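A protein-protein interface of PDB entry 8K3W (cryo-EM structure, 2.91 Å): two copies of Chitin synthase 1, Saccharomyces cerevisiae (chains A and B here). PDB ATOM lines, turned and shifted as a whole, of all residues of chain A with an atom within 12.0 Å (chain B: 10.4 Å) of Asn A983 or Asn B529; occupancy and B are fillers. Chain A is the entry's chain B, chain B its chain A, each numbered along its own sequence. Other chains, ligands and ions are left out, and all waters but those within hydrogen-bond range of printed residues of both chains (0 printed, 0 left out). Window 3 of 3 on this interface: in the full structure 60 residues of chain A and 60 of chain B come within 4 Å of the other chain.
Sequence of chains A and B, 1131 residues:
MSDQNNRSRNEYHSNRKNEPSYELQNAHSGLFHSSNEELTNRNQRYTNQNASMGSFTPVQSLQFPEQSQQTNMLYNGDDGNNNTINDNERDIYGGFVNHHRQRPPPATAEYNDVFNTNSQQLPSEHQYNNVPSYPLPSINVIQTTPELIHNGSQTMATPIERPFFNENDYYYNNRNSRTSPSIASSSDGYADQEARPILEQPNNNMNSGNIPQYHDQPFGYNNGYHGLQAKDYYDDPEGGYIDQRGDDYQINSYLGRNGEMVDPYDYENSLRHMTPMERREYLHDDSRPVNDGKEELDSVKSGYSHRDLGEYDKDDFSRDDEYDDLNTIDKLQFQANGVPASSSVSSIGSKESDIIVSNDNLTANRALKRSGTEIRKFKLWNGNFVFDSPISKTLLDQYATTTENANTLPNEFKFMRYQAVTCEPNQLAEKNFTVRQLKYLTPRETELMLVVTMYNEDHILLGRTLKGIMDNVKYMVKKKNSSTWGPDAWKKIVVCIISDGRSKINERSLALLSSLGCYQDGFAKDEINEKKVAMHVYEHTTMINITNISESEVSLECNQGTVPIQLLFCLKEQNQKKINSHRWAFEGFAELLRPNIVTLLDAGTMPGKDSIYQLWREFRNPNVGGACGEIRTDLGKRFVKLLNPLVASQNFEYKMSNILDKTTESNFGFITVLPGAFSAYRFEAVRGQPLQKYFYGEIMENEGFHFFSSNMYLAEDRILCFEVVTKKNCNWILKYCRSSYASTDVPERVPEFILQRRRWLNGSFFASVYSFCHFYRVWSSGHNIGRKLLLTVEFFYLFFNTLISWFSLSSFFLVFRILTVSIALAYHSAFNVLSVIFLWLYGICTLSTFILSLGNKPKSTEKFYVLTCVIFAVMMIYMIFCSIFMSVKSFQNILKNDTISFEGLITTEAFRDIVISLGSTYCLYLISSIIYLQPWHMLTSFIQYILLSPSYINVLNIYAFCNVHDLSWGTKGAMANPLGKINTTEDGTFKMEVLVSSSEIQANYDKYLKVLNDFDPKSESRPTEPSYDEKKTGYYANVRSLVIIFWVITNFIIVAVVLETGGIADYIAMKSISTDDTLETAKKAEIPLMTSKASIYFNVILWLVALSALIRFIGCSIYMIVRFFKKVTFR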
ATOM      1  N   LEU A 979      24.359  -2.025   0.072  1.00  0.00           N
ATOM      2  CA  LEU A 979      24.757  -2.289  -1.337  1.00  0.00           C
ATOM      3  C   LEU A 979      24.553  -1.029  -2.182  1.00  0.00           C
ATOM      4  O   LEU A 979      23.993  -0.048  -1.652  1.00  0.00           O
ATOM      5  CB  LEU A 979      23.914  -3.448  -1.877  1.00  0.00           C
ATOM      6  N   GLY A 980      24.988  -1.061  -3.445  1.00  0.00           N
ATOM      7  CA  GLY A 980      24.789   0.085  -4.355  1.00  0.00           C
ATOM      8  C   GLY A 980      25.458   1.352  -3.856  1.00  0.00           C
ATOM      9  O   GLY A 980      24.757   2.372  -3.732  1.00  0.00           O
ATOM     10  N   LYS A 981      26.764   1.301  -3.580  1.00  0.00           N
ATOM     11  CA  LYS A 981      27.499   2.531  -3.180  1.00  0.00           C
ATOM     12  C   LYS A 981      27.874   3.305  -4.448  1.00  0.00           C
ATOM     13  O   LYS A 981      29.078   3.564  -4.644  1.00  0.00           O
ATOM     14  CB  LYS A 981      28.741   2.172  -2.360  1.00  0.00           C
ATOM     15  N   ILE A 982      26.881   3.669  -5.265  1.00  0.00           N
ATOM     16  CA  ILE A 982      27.157   4.366  -6.557  1.00  0.00           C
ATOM     17  C   ILE A 982      27.567   5.812  -6.266  1.00  0.00           C
ATOM     18  O   ILE A 982      26.694   6.599  -5.859  1.00  0.00           O
ATOM     19  CB  ILE A 982      25.925   4.304  -7.481  1.00  0.00           C
ATOM     20  N   ASN A 983      28.844   6.144  -6.479  1.00  0.00           N
ATOM     21  CA  ASN A 983      29.330   7.533  -6.266  1.00  0.00           C
ATOM     22  C   ASN A 983      30.226   7.929  -7.445  1.00  0.00           C
ATOM     23  O   ASN A 983      31.436   8.128  -7.222  1.00  0.00           O
ATOM     24  CB  ASN A 983      30.058   7.676  -4.927  1.00  0.00           C
ATOM     25  N   THR A 984      29.650   8.039  -8.646  1.00  0.00           N
ATOM     26  CA  THR A 984      30.444   8.382  -9.857  1.00  0.00           C
ATOM     27  C   THR A 984      30.631   9.900  -9.936  1.00  0.00           C
ATOM     28  O   THR A 984      29.643  10.599 -10.235  1.00  0.00           O
ATOM     29  CB  THR A 984      29.780   7.835 -11.128  1.00  0.00           C
ATOM     30  N   THR A 985      31.852  10.383  -9.683  1.00  0.00           N
ATOM     31  CA  THR A 985      32.132  11.843  -9.715  1.00  0.00           C
ATOM     32  C   THR A 985      31.895  12.379 -11.131  1.00  0.00           C
ATOM     33  O   THR A 985      31.371  13.503 -11.253  1.00  0.00           O
ATOM     34  CB  THR A 985      33.558  12.142  -9.235  1.00  0.00           C
ATOM     35  N   GLU A 986      32.265  11.601 -12.152  1.00  0.00           N
ATOM     36  CA  GLU A 986      32.106  12.047 -13.563  1.00  0.00           C
ATOM     37  C   GLU A 986      30.729  11.614 -14.079  1.00  0.00           C
ATOM     38  O   GLU A 986      30.526  11.650 -15.309  1.00  0.00           O
ATOM     39  CB  GLU A 986      33.223  11.466 -14.432  1.00  0.00           C
ATOM     40  N   ASP A 987      29.832  11.213 -13.174  1.00  0.00           N
ATOM     41  CA  ASP A 987      28.474  10.758 -13.576  1.00  0.00           C
ATOM     42  C   ASP A 987      28.611   9.566 -14.530  1.00  0.00           C
ATOM     43  O   ASP A 987      27.815   9.483 -15.485  1.00  0.00           O
ATOM     44  CB  ASP A 987      27.663  11.899 -14.196  1.00  0.00           C
ATOM     45  N   GLY A 988      29.584   8.687 -14.276  1.00  0.00           N
ATOM     46  CA  GLY A 988      29.800   7.511 -15.141  1.00  0.00           C
ATOM     47  C   GLY A 988      28.648   6.527 -15.051  1.00  0.00           C
ATOM     48  O   GLY A 988      28.172   6.280 -13.926  1.00  0.00           O
ATOM     49  N   THR A 989      28.217   5.982 -16.193  1.00  0.00           N
ATOM     50  CA  THR A 989      27.111   4.988 -16.211  1.00  0.00           C
ATOM     51  C   THR A 989      27.688   3.591 -15.959  1.00  0.00           C
ATOM     52  O   THR A 989      27.921   2.866 -16.945  1.00  0.00           O
ATOM     53  CB  THR A 989      26.338   5.045 -17.534  1.00  0.00           C
ATOM     54  N   PHE A 990      27.904   3.235 -14.689  1.00  0.00           N
ATOM     55  CA  PHE A 990      28.508   1.919 -14.358  1.00  0.00           C
ATOM     56  C   PHE A 990      27.662   0.807 -14.983  1.00  0.00           C
ATOM     57  O   PHE A 990      28.224  -0.036 -15.709  1.00  0.00           O
ATOM     58  CB  PHE A 990      28.620   1.748 -12.841  1.00  0.00           C
ATOM     59  N   LYS A 991      26.352   0.812 -14.716  1.00  0.00           N
ATOM     60  CA  LYS A 991      25.446  -0.193 -15.333  1.00  0.00           C
ATOM     61  C   LYS A 991      25.286   0.131 -16.822  1.00  0.00           C
ATOM     62  O   LYS A 991      25.354  -0.806 -17.640  1.00  0.00           O
ATOM     63  CB  LYS A 991      24.090  -0.200 -14.623  1.00  0.00           C
ATOM     64  N   GLY B 383      21.411  16.018 -10.265  1.00  0.00           N
ATOM     65  CA  GLY B 383      22.309  15.677  -9.185  1.00  0.00           C
ATOM     66  C   GLY B 383      21.770  14.695  -8.172  1.00  0.00           C
ATOM     67  O   GLY B 383      22.369  14.548  -7.098  1.00  0.00           O
ATOM     68  N   ASN B 384      20.664  14.019  -8.465  1.00  0.00           N
ATOM     69  CA  ASN B 384      20.067  13.037  -7.566  1.00  0.00           C
ATOM     70  C   ASN B 384      19.796  11.753  -8.335  1.00  0.00           C
ATOM     71  O   ASN B 384      19.564  11.788  -9.547  1.00  0.00           O
ATOM     72  CB  ASN B 384      18.767  13.565  -6.952  1.00  0.00           C
ATOM     73  CG  ASN B 384      18.922  14.948  -6.354  1.00  0.00           C
ATOM     74  OD1 ASN B 384      19.960  15.280  -5.784  1.00  0.00           O
ATOM     75  ND2 ASN B 384      17.885  15.765  -6.483  1.00  0.00           N
ATOM     76  N   PHE B 385      19.841  10.624  -7.636  1.00  0.00           N
ATOM     77  CA  PHE B 385      19.592   9.340  -8.275  1.00  0.00           C
ATOM     78  C   PHE B 385      18.098   9.151  -8.518  1.00  0.00           C
ATOM     79  O   PHE B 385      17.289   9.313  -7.600  1.00  0.00           O
ATOM     80  CB  PHE B 385      20.139   8.214  -7.405  1.00  0.00           C
ATOM     81  CG  PHE B 385      20.049   6.861  -8.033  1.00  0.00           C
ATOM     82  CD1 PHE B 385      20.267   6.700  -9.387  1.00  0.00           C
ATOM     83  CD2 PHE B 385      19.750   5.747  -7.271  1.00  0.00           C
ATOM     84  CE1 PHE B 385      20.186   5.459  -9.968  1.00  0.00           C
ATOM     85  CE2 PHE B 385      19.667   4.505  -7.850  1.00  0.00           C
ATOM     86  CZ  PHE B 385      19.886   4.358  -9.199  1.00  0.00           C
ATOM     87  N   ALA B 420      16.407   8.540  -4.377  1.00  0.00           N
ATOM     88  CA  ALA B 420      17.273   8.327  -3.221  1.00  0.00           C
ATOM     89  C   ALA B 420      17.425   9.643  -2.471  1.00  0.00           C
ATOM     90  O   ALA B 420      18.221  10.499  -2.868  1.00  0.00           O
ATOM     91  CB  ALA B 420      18.629   7.781  -3.657  1.00  0.00           C
ATOM     92  N   THR B 422      18.840  11.803   0.202  1.00  0.00           N
ATOM     93  CA  THR B 422      20.035  11.787   1.028  1.00  0.00           C
ATOM     94  C   THR B 422      20.197  13.035   1.886  1.00  0.00           C
ATOM     95  O   THR B 422      21.288  13.265   2.417  1.00  0.00           O
ATOM     96  CB  THR B 422      21.279  11.607   0.148  1.00  0.00           C
ATOM     97  OG1 THR B 422      22.443  11.513   0.976  1.00  0.00           O
ATOM     98  CG2 THR B 422      21.430  12.773  -0.812  1.00  0.00           C
ATOM     99  N   PHE B 433      14.954  18.308  -4.881  1.00  0.00           N
ATOM    100  CA  PHE B 433      14.156  17.091  -4.860  1.00  0.00           C
ATOM    101  C   PHE B 433      12.703  17.457  -5.107  1.00  0.00           C
ATOM    102  O   PHE B 433      12.191  18.422  -4.537  1.00  0.00           O
ATOM    103  CB  PHE B 433      14.262  16.351  -3.526  1.00  0.00           C
ATOM    104  CG  PHE B 433      15.520  15.559  -3.369  1.00  0.00           C
ATOM    105  CD1 PHE B 433      15.467  14.193  -3.177  1.00  0.00           C
ATOM    106  CD2 PHE B 433      16.749  16.182  -3.363  1.00  0.00           C
ATOM    107  CE1 PHE B 433      16.618  13.456  -3.027  1.00  0.00           C
ATOM    108  CE2 PHE B 433      17.905  15.447  -3.200  1.00  0.00           C
ATOM    109  CZ  PHE B 433      17.835  14.083  -3.033  1.00  0.00           C
ATOM    110  N   LYS B 525      20.119   2.121  -3.628  1.00  0.00           N
ATOM    111  CA  LYS B 525      21.545   2.437  -3.347  1.00  0.00           C
ATOM    112  C   LYS B 525      21.683   2.905  -1.897  1.00  0.00           C
ATOM    113  O   LYS B 525      21.162   3.986  -1.582  1.00  0.00           O
ATOM    114  CB  LYS B 525      22.061   3.497  -4.327  1.00  0.00           C
ATOM    115  CG  LYS B 525      21.864   3.157  -5.796  1.00  0.00           C
ATOM    116  CD  LYS B 525      22.366   1.777  -6.157  1.00  0.00           C
ATOM    117  CE  LYS B 525      21.823   1.284  -7.482  1.00  0.00           C
ATOM    118  NZ  LYS B 525      20.343   1.221  -7.473  1.00  0.00           N
ATOM    119  N   ASP B 526      22.372   2.124  -1.065  1.00  0.00           N
ATOM    120  CA  ASP B 526      22.526   2.467   0.374  1.00  0.00           C
ATOM    121  C   ASP B 526      23.585   3.565   0.530  1.00  0.00           C
ATOM    122  O   ASP B 526      23.789   4.030   1.668  1.00  0.00           O
ATOM    123  CB  ASP B 526      22.867   1.230   1.207  1.00  0.00           C
ATOM    124  N   GLU B 527      24.235   3.953  -0.569  1.00  0.00           N
ATOM    125  CA  GLU B 527      25.298   4.988  -0.504  1.00  0.00           C
ATOM    126  C   GLU B 527      25.457   5.646  -1.877  1.00  0.00           C
ATOM    127  O   GLU B 527      25.504   4.906  -2.879  1.00  0.00           O
ATOM    128  CB  GLU B 527      26.616   4.354  -0.059  1.00  0.00           C
ATOM    129  CG  GLU B 527      27.774   5.332   0.007  1.00  0.00           C
ATOM    130  CD  GLU B 527      27.745   6.261   1.208  1.00  0.00           C
ATOM    131  OE1 GLU B 527      26.681   6.368   1.844  1.00  0.00           O
ATOM    132  OE2 GLU B 527      28.793   6.861   1.514  1.00  0.00           O
ATOM    133  N   ILE B 528      25.537   6.978  -1.915  1.00  0.00           N
ATOM    134  CA  ILE B 528      25.752   7.707  -3.201  1.00  0.00           C
ATOM    135  C   ILE B 528      26.587   8.955  -2.903  1.00  0.00           C
ATOM    136  O   ILE B 528      26.345   9.587  -1.859  1.00  0.00           O
ATOM    137  CB  ILE B 528      24.411   8.064  -3.873  1.00  0.00           C
ATOM    138  CG1 ILE B 528      23.574   6.819  -4.179  1.00  0.00           C
ATOM    139  CG2 ILE B 528      24.640   8.907  -5.118  1.00  0.00           C
ATOM    140  CD1 ILE B 528      22.241   7.120  -4.816  1.00  0.00           C
ATOM    141  N   ASN B 529      27.537   9.285  -3.783  1.00  0.00           N
ATOM    142  CA  ASN B 529      28.398  10.482  -3.587  1.00  0.00           C
ATOM    143  C   ASN B 529      29.069  10.396  -2.214  1.00  0.00           C
ATOM    144  O   ASN B 529      29.295  11.458  -1.603  1.00  0.00           O
ATOM    145  CB  ASN B 529      27.602  11.780  -3.748  1.00  0.00           C
ATOM    146  N   GLU B 530      29.366   9.178  -1.750  1.00  0.00           N
ATOM    147  CA  GLU B 530      30.001   8.985  -0.418  1.00  0.00           C
ATOM    148  C   GLU B 530      29.097   9.583   0.665  1.00  0.00           C
ATOM    149  O   GLU B 530      29.635  10.060   1.683  1.00  0.00           O
ATOM    150  CB  GLU B 530      31.391   9.626  -0.390  1.00  0.00           C
ATOM    151  N   LYS B 531      27.777   9.550   0.452  1.00  0.00           N
ATOM    152  CA  LYS B 531      26.812  10.102   1.440  1.00  0.00           C
ATOM    153  C   LYS B 531      25.673   9.096   1.626  1.00  0.00           C
ATOM    154  O   LYS B 531      25.189   8.568   0.608  1.00  0.00           O
ATOM    155  CB  LYS B 531      26.276  11.454   0.964  1.00  0.00           C
ATOM    156  N   LYS B 532      25.289   8.825   2.876  1.00  0.00           N
ATOM    157  CA  LYS B 532      24.254   7.792   3.148  1.00  0.00           C
ATOM    158  C   LYS B 532      22.869   8.321   2.777  1.00  0.00           C
ATOM    159  O   LYS B 532      22.479   9.375   3.314  1.00  0.00           O
ATOM    160  CB  LYS B 532      24.307   7.369   4.620  1.00  0.00           C
ATOM    161  CG  LYS B 532      25.520   6.536   5.017  1.00  0.00           C
ATOM    162  CD  LYS B 532      26.833   7.281   4.903  1.00  0.00           C
ATOM    163  CE  LYS B 532      28.040   6.391   5.114  1.00  0.00           C
ATOM    164  NZ  LYS B 532      29.308   7.136   4.930  1.00  0.00           N
ATOM    165  N   VAL B 533      22.163   7.621   1.887  1.00  0.00           N
ATOM    166  CA  VAL B 533      20.810   8.008   1.529  1.00  0.00           C
ATOM    167  C   VAL B 533      19.905   7.830   2.743  1.00  0.00           C
ATOM    168  O   VAL B 533      19.922   6.786   3.407  1.00  0.00           O
ATOM    169  CB  VAL B 533      20.335   7.195   0.312  1.00  0.00           C
ATOM    170  CG1 VAL B 533      20.406   5.719   0.597  1.00  0.00           C
ATOM    171  CG2 VAL B 533      18.929   7.585  -0.063  1.00  0.00           C
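Of the 15 printed residues of chain B, 6 touch a printed residue of chain A. Printed residues of chain B that touch a printed residue of chain A: Lys B525, Asp B526, Glu B527, Ile B528, Asn B529 and Glu B530. Hydrophobic or aromatic side chains of chain B that line the printed part of chain A: Ile B528. Of the 13 printed residues of chain A, 5 touch a printed residue of chain B. Along chain A the printed residues that touch a printed residue of chain B span positions 979 to 983. Among the printed residues, no Asp or Glu carboxylate lies within 4 Å of a Lys or Arg side-chain nitrogen of the other chain.
Lys B525 touches Leu A979 (C to O, 3.8 Å). CB of Lys B525 touches O of Gly A980, 3.0 Å away. Asp B526 touches Gly A980 (N to O, 3.6 Å). Lys A981 touches Glu B527. Ile A982 touches Ile B528 (O to CA, 3.0 Å). Asn A983 touches Asn B529. CB of Asn A983 touches N of Glu B530, at 3.6 Å.
Of the printed residues of chain B, Leu A979 touches Lys B525 (3.8 Å) and Asp B526 (2.8 Å). Printed residues of chain B within 4 Å of Ile A982: Glu B527 (3.0 Å), Ile B528 (3.0 Å) and Asn B529 (3.5 Å). No residue of chain B comes within 4 Å of Thr A984. Printed residues of chain A within 4 Å of Lys B525: Leu A979 and Gly A980. Of the printed residues of chain A, Glu B527 touches Gly A980, Lys A981 and Ile A982. Of the printed residues of chain A, Ile B528 touches Ile A982 (3.0 Å). Of the printed residues of chain A, Asn B529 touches Ile A982 (3.5 Å) and Asn A983 (3.2 Å). Of chain A, only Asn A983 (3.6 Å) comes within 4 Å of Glu B530. Lys B531 touches none of the printed residues of chain A. The nearest printed residue of chain A that does not touch Asp B526 is Lys A981 (5.1 Å).
No position is printed for both chains. Of the 11 pairs that touch across the chains among the printed residues, none has its exchanged pair printed and touching as well.
OE2 of Glu B527 sits at hydrogen-bond distance from N of Lys B531, at 3.1 Å. OE2 of Glu B527 lies within salt-bridge range of NZ of Lys B532 (3.5 Å).
The backbone NH (N) of Asp B526 sits at hydrogen-bond distance from the backbone carbonyl oxygen (O) of Leu A979 (2.8 Å). O of Glu B527 lies within hydrogen-bond range of N of Ile A982. O of Ile A982 lies within hydrogen-bond range of N of Asn B529 (3.5 Å). O of Glu B527 lies close to O of Gly A980 (2.8 Å).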
